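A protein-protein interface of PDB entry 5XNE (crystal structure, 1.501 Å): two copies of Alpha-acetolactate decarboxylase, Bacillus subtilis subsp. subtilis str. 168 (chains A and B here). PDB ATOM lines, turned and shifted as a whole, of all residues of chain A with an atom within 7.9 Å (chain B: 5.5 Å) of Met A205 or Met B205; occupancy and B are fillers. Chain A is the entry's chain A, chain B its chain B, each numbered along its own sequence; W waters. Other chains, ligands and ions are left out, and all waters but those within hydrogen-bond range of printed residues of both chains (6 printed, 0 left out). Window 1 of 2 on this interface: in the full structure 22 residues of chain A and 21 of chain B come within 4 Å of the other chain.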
ATOM      1  N   SER A   2     -28.874  21.843 -29.210  1.00  0.00           N
ATOM      2  CA  SER A   2     -27.523  22.240 -28.817  1.00  0.00           C
ATOM      3  C   SER A   2     -26.681  21.019 -28.480  1.00  0.00           C
ATOM      4  O   SER A   2     -25.795  21.072 -27.620  1.00  0.00           O
ATOM      5  CB  SER A   2     -27.549  23.200 -27.619  1.00  0.00           C
ATOM      6  OG  SER A   2     -26.296  23.870 -27.471  1.00  0.00           O
ATOM      7  N   GLN A   3     -26.951  19.908 -29.155  1.00  0.00           N
ATOM      8  CA  GLN A   3     -26.176  18.709 -28.886  1.00  0.00           C
ATOM      9  C   GLN A   3     -25.742  17.995 -30.149  1.00  0.00           C
ATOM     10  O   GLN A   3     -26.396  18.083 -31.196  1.00  0.00           O
ATOM     11  CB  GLN A   3     -26.972  17.733 -28.016  1.00  0.00           C
ATOM     12  CG  GLN A   3     -28.163  17.103 -28.728  1.00  0.00           C
ATOM     13  CD  GLN A   3     -28.862  16.035 -27.904  1.00  0.00           C
ATOM     14  OE1 GLN A   3     -28.682  15.947 -26.689  1.00  0.00           O
ATOM     15  NE2 GLN A   3     -29.675  15.221 -28.568  1.00  0.00           N
ATOM     16  N   ILE A   4     -24.633  17.280 -30.024  1.00  0.00           N
ATOM     17  CA  ILE A   4     -24.301  16.193 -30.938  1.00  0.00           C
ATOM     18  C   ILE A   4     -24.958  14.935 -30.376  1.00  0.00           C
ATOM     19  O   ILE A   4     -24.777  14.616 -29.194  1.00  0.00           O
ATOM     20  CB  ILE A   4     -22.787  15.967 -31.056  1.00  0.00           C
ATOM     21  CG1 ILE A   4     -22.052  17.273 -31.388  1.00  0.00           C
ATOM     22  CG2 ILE A   4     -22.495  14.865 -32.074  1.00  0.00           C
ATOM     23  CD1 ILE A   4     -22.412  17.857 -32.749  1.00  0.00           C
ATOM     24  N   TYR A   5     -25.736  14.239 -31.195  1.00  0.00           N
ATOM     25  CA  TYR A   5     -26.304  12.954 -30.800  1.00  0.00           C
ATOM     26  C   TYR A   5     -25.391  11.870 -31.346  1.00  0.00           C
ATOM     27  O   TYR A   5     -25.278  11.688 -32.564  1.00  0.00           O
ATOM     28  CB  TYR A   5     -27.732  12.767 -31.328  1.00  0.00           C
ATOM     29  CG  TYR A   5     -28.421  11.551 -30.757  1.00  0.00           C
ATOM     30  CD1 TYR A   5     -28.949  11.585 -29.476  1.00  0.00           C
ATOM     31  CD2 TYR A   5     -28.546  10.378 -31.496  1.00  0.00           C
ATOM     32  CE1 TYR A   5     -29.584  10.489 -28.925  1.00  0.00           C
ATOM     33  CE2 TYR A   5     -29.192   9.263 -30.950  1.00  0.00           C
ATOM     34  CZ  TYR A   5     -29.702   9.333 -29.664  1.00  0.00           C
ATOM     35  OH  TYR A   5     -30.342   8.255 -29.086  1.00  0.00           O
ATOM     36  N   GLN A   6     -24.715  11.177 -30.437  1.00  0.00           N
ATOM     37  CA  GLN A   6     -23.667  10.220 -30.784  1.00  0.00           C
ATOM     38  C   GLN A   6     -24.145   8.789 -30.570  1.00  0.00           C
ATOM     39  O   GLN A   6     -24.450   8.391 -29.439  1.00  0.00           O
ATOM     40  CB  GLN A   6     -22.413  10.502 -29.955  1.00  0.00           C
ATOM     41  CG  GLN A   6     -21.270   9.549 -30.187  1.00  0.00           C
ATOM     42  CD  GLN A   6     -20.843   9.509 -31.627  1.00  0.00           C
ATOM     43  OE1 GLN A   6     -20.579  10.548 -32.230  1.00  0.00           O
ATOM     44  NE2 GLN A   6     -20.769   8.308 -32.198  1.00  0.00           N
ATOM     45  N   VAL A   7     -24.220   8.022 -31.658  1.00  0.00           N
ATOM     46  CA  VAL A   7     -24.654   6.628 -31.594  1.00  0.00           C
ATOM     47  C   VAL A   7     -23.423   5.726 -31.453  1.00  0.00           C
ATOM     48  O   VAL A   7     -22.619   5.595 -32.381  1.00  0.00           O
ATOM     49  CB  VAL A   7     -25.476   6.250 -32.846  1.00  0.00           C
ATOM     50  CG1 VAL A   7     -25.742   4.746 -32.892  1.00  0.00           C
ATOM     51  CG2 VAL A   7     -26.794   7.019 -32.862  1.00  0.00           C
ATOM     52  N   SER A   8     -23.273   5.156 -30.251  1.00  0.00           N
ATOM     53  CA  SER A   8     -22.190   4.232 -29.881  1.00  0.00           C
ATOM     54  C   SER A   8     -20.787   4.842 -30.004  1.00  0.00           C
ATOM     55  O   SER A   8     -20.639   6.073 -30.089  1.00  0.00           O
ATOM     56  CB  SER A   8     -22.274   2.944 -30.718  1.00  0.00           C
ATOM     57  OG  SER A   8     -21.519   1.896 -30.114  1.00  0.00           O
ATOM     58  N   SER A  74     -23.307   9.982 -36.077  1.00  0.00           N
ATOM     59  CA  SER A  74     -23.350  11.218 -35.301  1.00  0.00           C
ATOM     60  C   SER A  74     -24.341  12.164 -35.987  1.00  0.00           C
ATOM     61  O   SER A  74     -24.272  12.317 -37.207  1.00  0.00           O
ATOM     62  CB  SER A  74     -21.963  11.884 -35.230  1.00  0.00           C
ATOM     63  OG  SER A  74     -20.929  10.986 -34.848  1.00  0.00           O
ATOM     64  N   PHE A 109     -17.736  21.076 -29.461  1.00  0.00           N
ATOM     65  CA  PHE A 109     -18.081  20.277 -30.645  1.00  0.00           C
ATOM     66  C   PHE A 109     -18.600  21.176 -31.761  1.00  0.00           C
ATOM     67  O   PHE A 109     -19.332  22.130 -31.490  1.00  0.00           O
ATOM     68  CB  PHE A 109     -19.149  19.239 -30.299  1.00  0.00           C
ATOM     69  CG  PHE A 109     -18.675  18.162 -29.356  1.00  0.00           C
ATOM     70  CD1 PHE A 109     -18.569  18.404 -27.986  1.00  0.00           C
ATOM     71  CD2 PHE A 109     -18.353  16.899 -29.838  1.00  0.00           C
ATOM     72  CE1 PHE A 109     -18.123  17.400 -27.120  1.00  0.00           C
ATOM     73  CE2 PHE A 109     -17.914  15.893 -28.974  1.00  0.00           C
ATOM     74  CZ  PHE A 109     -17.805  16.150 -27.624  1.00  0.00           C
ATOM     75  N   THR A 160     -14.275  17.261 -33.406  1.00  0.00           N
ATOM     76  CA  THR A 160     -14.442  16.669 -32.089  1.00  0.00           C
ATOM     77  C   THR A 160     -13.229  16.963 -31.211  1.00  0.00           C
ATOM     78  O   THR A 160     -12.098  16.782 -31.656  1.00  0.00           O
ATOM     79  CB  THR A 160     -14.652  15.157 -32.219  1.00  0.00           C
ATOM     80  OG1 THR A 160     -15.879  14.922 -32.929  1.00  0.00           O
ATOM     81  CG2 THR A 160     -14.712  14.487 -30.860  1.00  0.00           C
ATOM     82  N   PRO A 161     -13.464  17.446 -29.977  1.00  0.00           N
ATOM     83  CA  PRO A 161     -12.359  17.698 -29.042  1.00  0.00           C
ATOM     84  C   PRO A 161     -11.590  16.440 -28.691  1.00  0.00           C
ATOM     85  O   PRO A 161     -12.161  15.339 -28.697  1.00  0.00           O
ATOM     86  CB  PRO A 161     -13.065  18.244 -27.786  1.00  0.00           C
ATOM     87  CG  PRO A 161     -14.376  18.720 -28.242  1.00  0.00           C
ATOM     88  CD  PRO A 161     -14.764  17.819 -29.403  1.00  0.00           C
ATOM     89  N   TYR A 163     -10.670  15.174 -25.905  1.00  0.00           N
ATOM     90  CA  TYR A 163     -11.159  14.380 -24.772  1.00  0.00           C
ATOM     91  C   TYR A 163     -12.243  13.361 -25.163  1.00  0.00           C
ATOM     92  O   TYR A 163     -12.535  12.444 -24.398  1.00  0.00           O
ATOM     93  CB  TYR A 163     -11.665  15.286 -23.637  1.00  0.00           C
ATOM     94  CG  TYR A 163     -12.766  16.250 -24.001  1.00  0.00           C
ATOM     95  CD1 TYR A 163     -14.069  15.804 -24.265  1.00  0.00           C
ATOM     96  CD2 TYR A 163     -12.518  17.620 -24.049  1.00  0.00           C
ATOM     97  CE1 TYR A 163     -15.077  16.692 -24.596  1.00  0.00           C
ATOM     98  CE2 TYR A 163     -13.524  18.513 -24.364  1.00  0.00           C
ATOM     99  CZ  TYR A 163     -14.805  18.048 -24.635  1.00  0.00           C
ATOM    100  OH  TYR A 163     -15.798  18.921 -24.962  1.00  0.00           O
ATOM    101  N   ALA A 164     -12.811  13.489 -26.360  1.00  0.00           N
ATOM    102  CA  ALA A 164     -13.829  12.526 -26.790  1.00  0.00           C
ATOM    103  C   ALA A 164     -13.283  11.523 -27.809  1.00  0.00           C
ATOM    104  O   ALA A 164     -14.051  10.716 -28.370  1.00  0.00           O
ATOM    105  CB  ALA A 164     -15.053  13.249 -27.351  1.00  0.00           C
ATOM    106  N   ILE A 167     -14.679   7.805 -28.273  1.00  0.00           N
ATOM    107  CA  ILE A 167     -16.121   7.863 -28.461  1.00  0.00           C
ATOM    108  C   ILE A 167     -16.394   8.237 -29.913  1.00  0.00           C
ATOM    109  O   ILE A 167     -17.034   7.481 -30.653  1.00  0.00           O
ATOM    110  CB  ILE A 167     -16.794   8.858 -27.514  1.00  0.00           C
ATOM    111  CG1 ILE A 167     -16.713   8.325 -26.080  1.00  0.00           C
ATOM    112  CG2 ILE A 167     -18.249   9.075 -27.932  1.00  0.00           C
ATOM    113  CD1 ILE A 167     -17.128   9.349 -25.033  1.00  0.00           C
ATOM    114  N   ALA A 168     -15.889   9.389 -30.326  1.00  0.00           N
ATOM    115  CA  ALA A 168     -15.919   9.773 -31.732  1.00  0.00           C
ATOM    116  C   ALA A 168     -14.484   9.866 -32.242  1.00  0.00           C
ATOM    117  O   ALA A 168     -13.558   9.338 -31.615  1.00  0.00           O
ATOM    118  CB  ALA A 168     -16.661  11.084 -31.911  1.00  0.00           C
ATOM    119  N   LYS A 202     -21.797  23.335 -30.850  1.00  0.00           N
ATOM    120  CA  LYS A 202     -22.647  22.590 -29.920  1.00  0.00           C
ATOM    121  C   LYS A 202     -21.998  22.457 -28.530  1.00  0.00           C
ATOM    122  O   LYS A 202     -20.793  22.181 -28.431  1.00  0.00           O
ATOM    123  CB  LYS A 202     -22.968  21.200 -30.492  1.00  0.00           C
ATOM    124  CG  LYS A 202     -23.780  21.225 -31.799  1.00  0.00           C
ATOM    125  CD  LYS A 202     -25.078  21.999 -31.611  1.00  0.00           C
ATOM    126  CE  LYS A 202     -25.924  22.026 -32.871  1.00  0.00           C
ATOM    127  NZ  LYS A 202     -25.116  22.525 -33.973  1.00  0.00           N
ATOM    128  N   MET A 203     -22.803  22.640 -27.475  1.00  0.00           N
ATOM    129  CA  MET A 203     -22.311  22.613 -26.090  1.00  0.00           C
ATOM    130  C   MET A 203     -22.602  21.307 -25.363  1.00  0.00           C
ATOM    131  O   MET A 203     -22.275  21.168 -24.193  1.00  0.00           O
ATOM    132  CB  MET A 203     -22.924  23.756 -25.272  1.00  0.00           C
ATOM    133  CG  MET A 203     -22.702  25.134 -25.844  1.00  0.00           C
ATOM    134  SD  MET A 203     -20.948  25.505 -25.969  1.00  0.00           S
ATOM    135  CE  MET A 203     -20.545  25.911 -24.258  1.00  0.00           C
ATOM    136  N   ASN A 204     -23.259  20.371 -26.042  1.00  0.00           N
ATOM    137  CA  ASN A 204     -23.588  19.080 -25.452  1.00  0.00           C
ATOM    138  C   ASN A 204     -23.216  17.956 -26.392  1.00  0.00           C
ATOM    139  O   ASN A 204     -23.324  18.101 -27.611  1.00  0.00           O
ATOM    140  CB  ASN A 204     -25.088  18.937 -25.143  1.00  0.00           C
ATOM    141  CG  ASN A 204     -25.570  19.853 -24.037  1.00  0.00           C
ATOM    142  OD1 ASN A 204     -25.700  19.442 -22.871  1.00  0.00           O
ATOM    143  ND2 ASN A 204     -25.878  21.090 -24.403  1.00  0.00           N
ATOM    144  N   MET A 205     -22.794  16.834 -25.827  1.00  0.00           N
ATOM    145  CA  MET A 205     -22.714  15.599 -26.591  1.00  0.00           C
ATOM    146  C   MET A 205     -23.508  14.548 -25.844  1.00  0.00           C
ATOM    147  O   MET A 205     -23.201  14.267 -24.679  1.00  0.00           O
ATOM    148  CB  MET A 205     -21.281  15.119 -26.776  1.00  0.00           C
ATOM    149  CG  MET A 205     -21.255  13.774 -27.498  1.00  0.00           C
ATOM    150  SD  MET A 205     -19.800  12.797 -27.186  1.00  0.00           S
ATOM    151  CE  MET A 205     -19.867  12.609 -25.411  1.00  0.00           C
ATOM    152  N   ASN A 206     -24.512  13.971 -26.499  1.00  0.00           N
ATOM    153  CA  ASN A 206     -25.252  12.879 -25.873  1.00  0.00           C
ATOM    154  C   ASN A 206     -24.891  11.564 -26.517  1.00  0.00           C
ATOM    155  O   ASN A 206     -25.229  11.327 -27.679  1.00  0.00           O
ATOM    156  CB  ASN A 206     -26.763  13.046 -25.953  1.00  0.00           C
ATOM    157  CG  ASN A 206     -27.491  11.869 -25.268  1.00  0.00           C
ATOM    158  OD1 ASN A 206     -27.748  11.909 -24.078  1.00  0.00           O
ATOM    159  ND2 ASN A 206     -27.735  10.788 -26.016  1.00  0.00           N
ATOM    160  N   LEU A 207     -24.217  10.725 -25.743  1.00  0.00           N
ATOM    161  CA  LEU A 207     -23.812   9.398 -26.189  1.00  0.00           C
ATOM    162  C   LEU A 207     -24.892   8.374 -25.879  1.00  0.00           C
ATOM    163  O   LEU A 207     -25.279   8.210 -24.720  1.00  0.00           O
ATOM    164  CB  LEU A 207     -22.504   9.004 -25.510  1.00  0.00           C
ATOM    165  CG  LEU A 207     -22.044   7.566 -25.715  1.00  0.00           C
ATOM    166  CD1 LEU A 207     -21.794   7.254 -27.192  1.00  0.00           C
ATOM    167  CD2 LEU A 207     -20.791   7.308 -24.893  1.00  0.00           C
ATOM    168  N   ARG A 208     -25.374   7.698 -26.919  1.00  0.00           N
ATOM    169  CA  ARG A 208     -26.362   6.625 -26.771  1.00  0.00           C
ATOM    170  C   ARG A 208     -25.705   5.275 -27.030  1.00  0.00           C
ATOM    171  O   ARG A 208     -25.162   5.039 -28.105  1.00  0.00           O
ATOM    172  CB  ARG A 208     -27.522   6.849 -27.735  1.00  0.00           C
ATOM    173  CG  ARG A 208     -28.477   5.673 -27.873  1.00  0.00           C
ATOM    174  CD  ARG A 208     -29.172   5.342 -26.559  1.00  0.00           C
ATOM    175  NE  ARG A 208     -30.451   4.681 -26.816  1.00  0.00           N
ATOM    176  CZ  ARG A 208     -30.581   3.413 -27.192  1.00  0.00           C
ATOM    177  NH1 ARG A 208     -29.515   2.654 -27.361  1.00  0.00           N
ATOM    178  NH2 ARG A 208     -31.788   2.902 -27.409  1.00  0.00           N
ATOM    179  N   LEU A 209     -25.735   4.397 -26.034  1.00  0.00           N
ATOM    180  CA  LEU A 209     -25.149   3.063 -26.187  1.00  0.00           C
ATOM    181  C   LEU A 209     -26.192   2.070 -26.689  1.00  0.00           C
ATOM    182  O   LEU A 209     -27.340   2.109 -26.265  1.00  0.00           O
ATOM    183  CB  LEU A 209     -24.571   2.586 -24.852  1.00  0.00           C
ATOM    184  CG  LEU A 209     -23.630   3.617 -24.205  1.00  0.00           C
ATOM    185  CD1 LEU A 209     -23.212   3.167 -22.801  1.00  0.00           C
ATOM    186  CD2 LEU A 209     -22.442   3.821 -25.131  1.00  0.00           C
ATOM    187  N   GLN B   3     -29.988   8.404 -18.307  1.00  0.00           N
ATOM    188  CA  GLN B   3     -28.683   8.976 -18.611  1.00  0.00           C
ATOM    189  C   GLN B   3     -27.880   9.347 -17.379  1.00  0.00           C
ATOM    190  O   GLN B   3     -28.435   9.598 -16.305  1.00  0.00           O
ATOM    191  CB  GLN B   3     -28.839  10.229 -19.473  1.00  0.00           C
ATOM    192  CG  GLN B   3     -29.574  11.368 -18.760  1.00  0.00           C
ATOM    193  CD  GLN B   3     -29.619  12.663 -19.555  1.00  0.00           C
ATOM    194  OE1 GLN B   3     -29.474  12.668 -20.774  1.00  0.00           O
ATOM    195  NE2 GLN B   3     -29.836  13.774 -18.857  1.00  0.00           N
ATOM    196  N   ILE B   4     -26.570   9.398 -17.563  1.00  0.00           N
ATOM    197  CA  ILE B   4     -25.696  10.158 -16.677  1.00  0.00           C
ATOM    198  C   ILE B   4     -25.638  11.580 -17.235  1.00  0.00           C
ATOM    199  O   ILE B   4     -25.364  11.770 -18.427  1.00  0.00           O
ATOM    200  CB  ILE B   4     -24.268   9.580 -16.609  1.00  0.00           C
ATOM    201  CG1 ILE B   4     -24.282   8.076 -16.283  1.00  0.00           C
ATOM    202  CG2 ILE B   4     -23.408  10.387 -15.620  1.00  0.00           C
ATOM    203  CD1 ILE B   4     -24.842   7.744 -14.914  1.00  0.00           C
ATOM    204  N   GLN B   6     -23.485  14.676 -17.216  1.00  0.00           N
ATOM    205  CA  GLN B   6     -22.084  14.956 -16.922  1.00  0.00           C
ATOM    206  C   GLN B   6     -21.774  16.430 -17.129  1.00  0.00           C
ATOM    207  O   GLN B   6     -21.874  16.935 -18.251  1.00  0.00           O
ATOM    208  CB  GLN B   6     -21.187  14.091 -17.809  1.00  0.00           C
ATOM    209  CG  GLN B   6     -19.710  14.305 -17.615  1.00  0.00           C
ATOM    210  CD  GLN B   6     -19.278  14.108 -16.184  1.00  0.00           C
ATOM    211  OE1 GLN B   6     -19.558  13.075 -15.579  1.00  0.00           O
ATOM    212  NE2 GLN B   6     -18.580  15.097 -15.628  1.00  0.00           N
ATOM    213  N   PHE B 109     -22.609   2.609 -18.327  1.00  0.00           N
ATOM    214  CA  PHE B 109     -22.453   3.472 -17.148  1.00  0.00           C
ATOM    215  C   PHE B 109     -23.320   2.955 -16.007  1.00  0.00           C
ATOM    216  O   PHE B 109     -24.446   2.516 -16.247  1.00  0.00           O
ATOM    217  CB  PHE B 109     -22.855   4.911 -17.480  1.00  0.00           C
ATOM    218  CG  PHE B 109     -21.925   5.604 -18.453  1.00  0.00           C
ATOM    219  CD1 PHE B 109     -22.010   5.360 -19.818  1.00  0.00           C
ATOM    220  CD2 PHE B 109     -20.976   6.512 -17.994  1.00  0.00           C
ATOM    221  CE1 PHE B 109     -21.141   6.000 -20.710  1.00  0.00           C
ATOM    222  CE2 PHE B 109     -20.116   7.159 -18.885  1.00  0.00           C
ATOM    223  CZ  PHE B 109     -20.204   6.897 -20.231  1.00  0.00           C
ATOM    224  N   ALA B 164     -14.622   6.625 -21.697  1.00  0.00           N
ATOM    225  CA  ALA B 164     -14.978   7.975 -21.225  1.00  0.00           C
ATOM    226  C   ALA B 164     -13.958   8.540 -20.237  1.00  0.00           C
ATOM    227  O   ALA B 164     -14.181   9.613 -19.650  1.00  0.00           O
ATOM    228  CB  ALA B 164     -16.372   7.977 -20.606  1.00  0.00           C
ATOM    229  N   ILE B 167     -13.232  12.457 -19.780  1.00  0.00           N
ATOM    230  CA  ILE B 167     -14.490  13.148 -19.534  1.00  0.00           C
ATOM    231  C   ILE B 167     -14.866  12.934 -18.072  1.00  0.00           C
ATOM    232  O   ILE B 167     -14.999  13.894 -17.311  1.00  0.00           O
ATOM    233  CB  ILE B 167     -15.611  12.661 -20.450  1.00  0.00           C
ATOM    234  CG1 ILE B 167     -15.312  13.101 -21.887  1.00  0.00           C
ATOM    235  CG2 ILE B 167     -16.953  13.214 -19.979  1.00  0.00           C
ATOM    236  CD1 ILE B 167     -16.198  12.425 -22.927  1.00  0.00           C
ATOM    237  N   MET B 203     -27.829   3.877 -20.121  1.00  0.00           N
ATOM    238  CA  MET B 203     -27.443   3.662 -21.525  1.00  0.00           C
ATOM    239  C   MET B 203     -27.052   4.934 -22.255  1.00  0.00           C
ATOM    240  O   MET B 203     -26.743   4.895 -23.439  1.00  0.00           O
ATOM    241  CB  MET B 203     -28.587   3.012 -22.310  1.00  0.00           C
ATOM    242  CG  MET B 203     -29.095   1.721 -21.728  1.00  0.00           C
ATOM    243  SD  MET B 203     -27.796   0.481 -21.698  1.00  0.00           S
ATOM    244  CE  MET B 203     -27.742  -0.026 -23.430  1.00  0.00           C
ATOM    245  N   ASN B 204     -27.116   6.069 -21.563  1.00  0.00           N
ATOM    246  CA  ASN B 204     -26.769   7.351 -22.157  1.00  0.00           C
ATOM    247  C   ASN B 204     -25.830   8.119 -21.249  1.00  0.00           C
ATOM    248  O   ASN B 204     -25.958   8.045 -20.028  1.00  0.00           O
ATOM    249  CB  ASN B 204     -28.004   8.237 -22.398  1.00  0.00           C
ATOM    250  CG  ASN B 204     -28.924   7.712 -23.483  1.00  0.00           C
ATOM    251  OD1 ASN B 204     -28.851   8.136 -24.650  1.00  0.00           O
ATOM    252  ND2 ASN B 204     -29.825   6.819 -23.097  1.00  0.00           N
ATOM    253  N   MET B 205     -24.910   8.870 -21.843  1.00  0.00           N
ATOM    254  CA  MET B 205     -24.178   9.888 -21.098  1.00  0.00           C
ATOM    255  C   MET B 205     -24.363  11.207 -21.822  1.00  0.00           C
ATOM    256  O   MET B 205     -24.008  11.303 -23.006  1.00  0.00           O
ATOM    257  CB  MET B 205     -22.690   9.576 -20.990  1.00  0.00           C
ATOM    258  CG  MET B 205     -21.949  10.716 -20.289  1.00  0.00           C
ATOM    259  SD  MET B 205     -20.196  10.779 -20.604  1.00  0.00           S
ATOM    260  CE  MET B 205     -20.161  10.944 -22.380  1.00  0.00           C
ATOM    261  N   ASN B 206     -24.897  12.213 -21.134  1.00  0.00           N
ATOM    262  CA  ASN B 206     -24.997  13.534 -21.745  1.00  0.00           C
ATOM    263  C   ASN B 206     -23.976  14.465 -21.133  1.00  0.00           C
ATOM    264  O   ASN B 206     -24.099  14.839 -19.969  1.00  0.00           O
ATOM    265  CB  ASN B 206     -26.370  14.171 -21.601  1.00  0.00           C
ATOM    266  CG  ASN B 206     -26.406  15.573 -22.249  1.00  0.00           C
ATOM    267  OD1 ASN B 206     -26.674  15.705 -23.429  1.00  0.00           O
ATOM    268  ND2 ASN B 206     -26.048  16.601 -21.480  1.00  0.00           N
ATOM    269  N   LEU B 207     -22.979  14.825 -21.930  1.00  0.00           N
ATOM    270  CA  LEU B 207     -21.956  15.777 -21.510  1.00  0.00           C
ATOM    271  C   LEU B 207     -22.373  17.211 -21.805  1.00  0.00           C
ATOM    272  O   LEU B 207     -22.659  17.557 -22.956  1.00  0.00           O
ATOM    273  CB  LEU B 207     -20.642  15.460 -22.222  1.00  0.00           C
ATOM    274  CG  LEU B 207     -19.503  16.462 -22.063  1.00  0.00           C
ATOM    275  CD1 LEU B 207     -19.064  16.569 -20.609  1.00  0.00           C
ATOM    276  CD2 LEU B 207     -18.340  16.046 -22.946  1.00  0.00           C
ATOM    277  N   ARG B 208     -22.409  18.036 -20.758  1.00  0.00           N
ATOM    278  CA  ARG B 208     -22.712  19.468 -20.885  1.00  0.00           C
ATOM    279  C   ARG B 208     -21.452  20.295 -20.650  1.00  0.00           C
ATOM    280  O   ARG B 208     -20.834  20.219 -19.582  1.00  0.00           O
ATOM    281  CB  ARG B 208     -23.793  19.862 -19.887  1.00  0.00           C
ATOM    282  CG  ARG B 208     -23.993  21.361 -19.720  1.00  0.00           C
ATOM    283  CD  ARG B 208     -24.416  22.005 -21.033  1.00  0.00           C
ATOM    284  NE  ARG B 208     -25.174  23.234 -20.802  1.00  0.00           N
ATOM    285  CZ  ARG B 208     -24.631  24.392 -20.443  1.00  0.00           C
ATOM    286  NH1 ARG B 208     -23.325  24.486 -20.264  1.00  0.00           N
ATOM    287  NH2 ARG B 208     -25.401  25.459 -20.253  1.00  0.00           N
HETATM  288  O   HOH W   1     -27.440  22.905 -22.950  1.00  0.00           O
HETATM  289  O   HOH W   2     -28.192  17.430 -24.597  1.00  0.00           O
HETATM  290  O   HOH W   3     -30.927   8.466 -26.464  1.00  0.00           O
HETATM  291  O   HOH W   4     -32.143   6.059 -24.653  1.00  0.00           O
HETATM  292  O   HOH W   5     -29.824  11.147 -22.868  1.00  0.00           O
HETATM  293  O   HOH W   6     -13.448  10.548 -22.750  1.00  0.00           O
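The backbone carbonyl oxygen (O) of Met B203 sits at hydrogen-bond distance from the backbone NH (N) of Leu A209, 2.8 Å away.
The side-chain amide oxygen of Asn B204 lies within hydrogen-bond range of the side-chain amide nitrogen of Asn A206 (3.2 Å).
The backbone carbonyl oxygen (O) of Met B205 sits at hydrogen-bond distance from the backbone NH (N) of Leu A207 (2.8 Å).
The side-chain amide nitrogen of Asn B206 sits at hydrogen-bond distance from the side-chain amide oxygen of Asn A204.
The backbone NH (N) of Leu B207 is in hydrogen-bond range of the backbone carbonyl oxygen (O) of Met A205 (2.8 Å).
The backbone carbonyl oxygen (O) of Met B205 lies close to the backbone carbonyl oxygen (O) of Met A205 (3.5 Å).
N of Ile B4 sits at hydrogen-bond distance from O of Asn B204 (2.9 Å).
O of Gln B6 lies within hydrogen-bond range of N of Arg B208.
The backbone carbonyl oxygen of Ser A2 lies within hydrogen-bond range of the backbone NH of Met A203.
N of Asn A204 is in hydrogen-bond range of O of Ser A2, 3.1 Å away.
The backbone carbonyl oxygen (O) of Ile A4 sits at hydrogen-bond distance from the backbone NH (N) of Asn A206 (2.8 Å).
O of Arg A208 lies within hydrogen-bond range of N of Ser A8, at 2.9 Å.
O of Tyr A163 touches CG1 of Ile B167, 3.8 Å away.
CD1 of Ile A167 touches CD1 of Ile B167 (3.8 Å).
CA of Asn A204 touches O of Leu B207 (3.1 Å).
Arg B208 touches Asn A204.
OD1 of Asn A206 touches OE1 of Gln B3, at 3.8 Å.
CA of Asn A206 touches O of Met B205, 3.5 Å away.
Asn B206 touches Asn A206 (CB to OD1, 3.6 Å).
Leu A207 touches Met B203 (O to O, 3.8 Å).
CA of Asn B204 touches O of Leu A207, at 3.1 Å.
Asn B204 touches Arg A208 (OD1 to CD, 3.4 Å).
Ser A8 touches none of the printed residues of chain B.
Ala A164 touches none of the printed residues of chain B.
Met A205 touches just these residues of chain B: Met B205, Asn B206 and Leu B207.
Of the printed residues of chain B, Leu A207 touches Met B203, Asn B204 and Met B205.
Of the printed residues of chain A, Asn B204 touches Asn A206 (3.2 Å), Leu A207 (3.1 Å) and Arg A208 (3.4 Å).
Of chain A, only Met A205, Asn A206 and Leu A207 come within 4 Å of Met B205.
Of the 23 printed residues of chain A, 10 touch a printed residue of chain B.
Hydrophobic or aromatic side chains of chain A that line the printed part of chain B: Tyr A163, Ile A167, Met A205, Leu A207 and Leu A209.
Hydrophobic or aromatic side chains of chain B within 4 Å of the printed part of chain A: Phe B109, Ile B167, Met B203, Met B205 and Leu B207.
Asn A204 touches Leu B207, and with the chains exchanged Leu A207 touches Asn B204.
Asn A204 touches Arg B208, and with the chains exchanged Arg A208 touches Asn B204.
Met B205 touches its own counterpart, Met A205.
Met A205 touches Asn B206, and with the chains exchanged Asn A206 touches Met B205.
Water W5 bridges OD1 of Asn A206 and OE1 of Gln B3.
Water W2 bridges OD1 of Asn B206 and OE1 of Gln A3.
Water W6 bridges the backbone carbonyl oxygen (O) of Tyr A163 and the backbone carbonyl oxygen (O) of Ala B164.
Water W3 lies within hydrogen-bond range of OH of Tyr A5 (2.7 Å) and OD1 of Asn B204 (2.8 Å).
Water W1 lies within hydrogen-bond range of the side-chain amide nitrogen of Asn A204 (2.8 Å) and the guanidinium group of Arg B208 (3.1 Å).
Water W4 bridges the side-chain amide nitrogen of Asn B204 (2.9 Å) and the guanidinium group of Arg A208 (3.1 Å).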
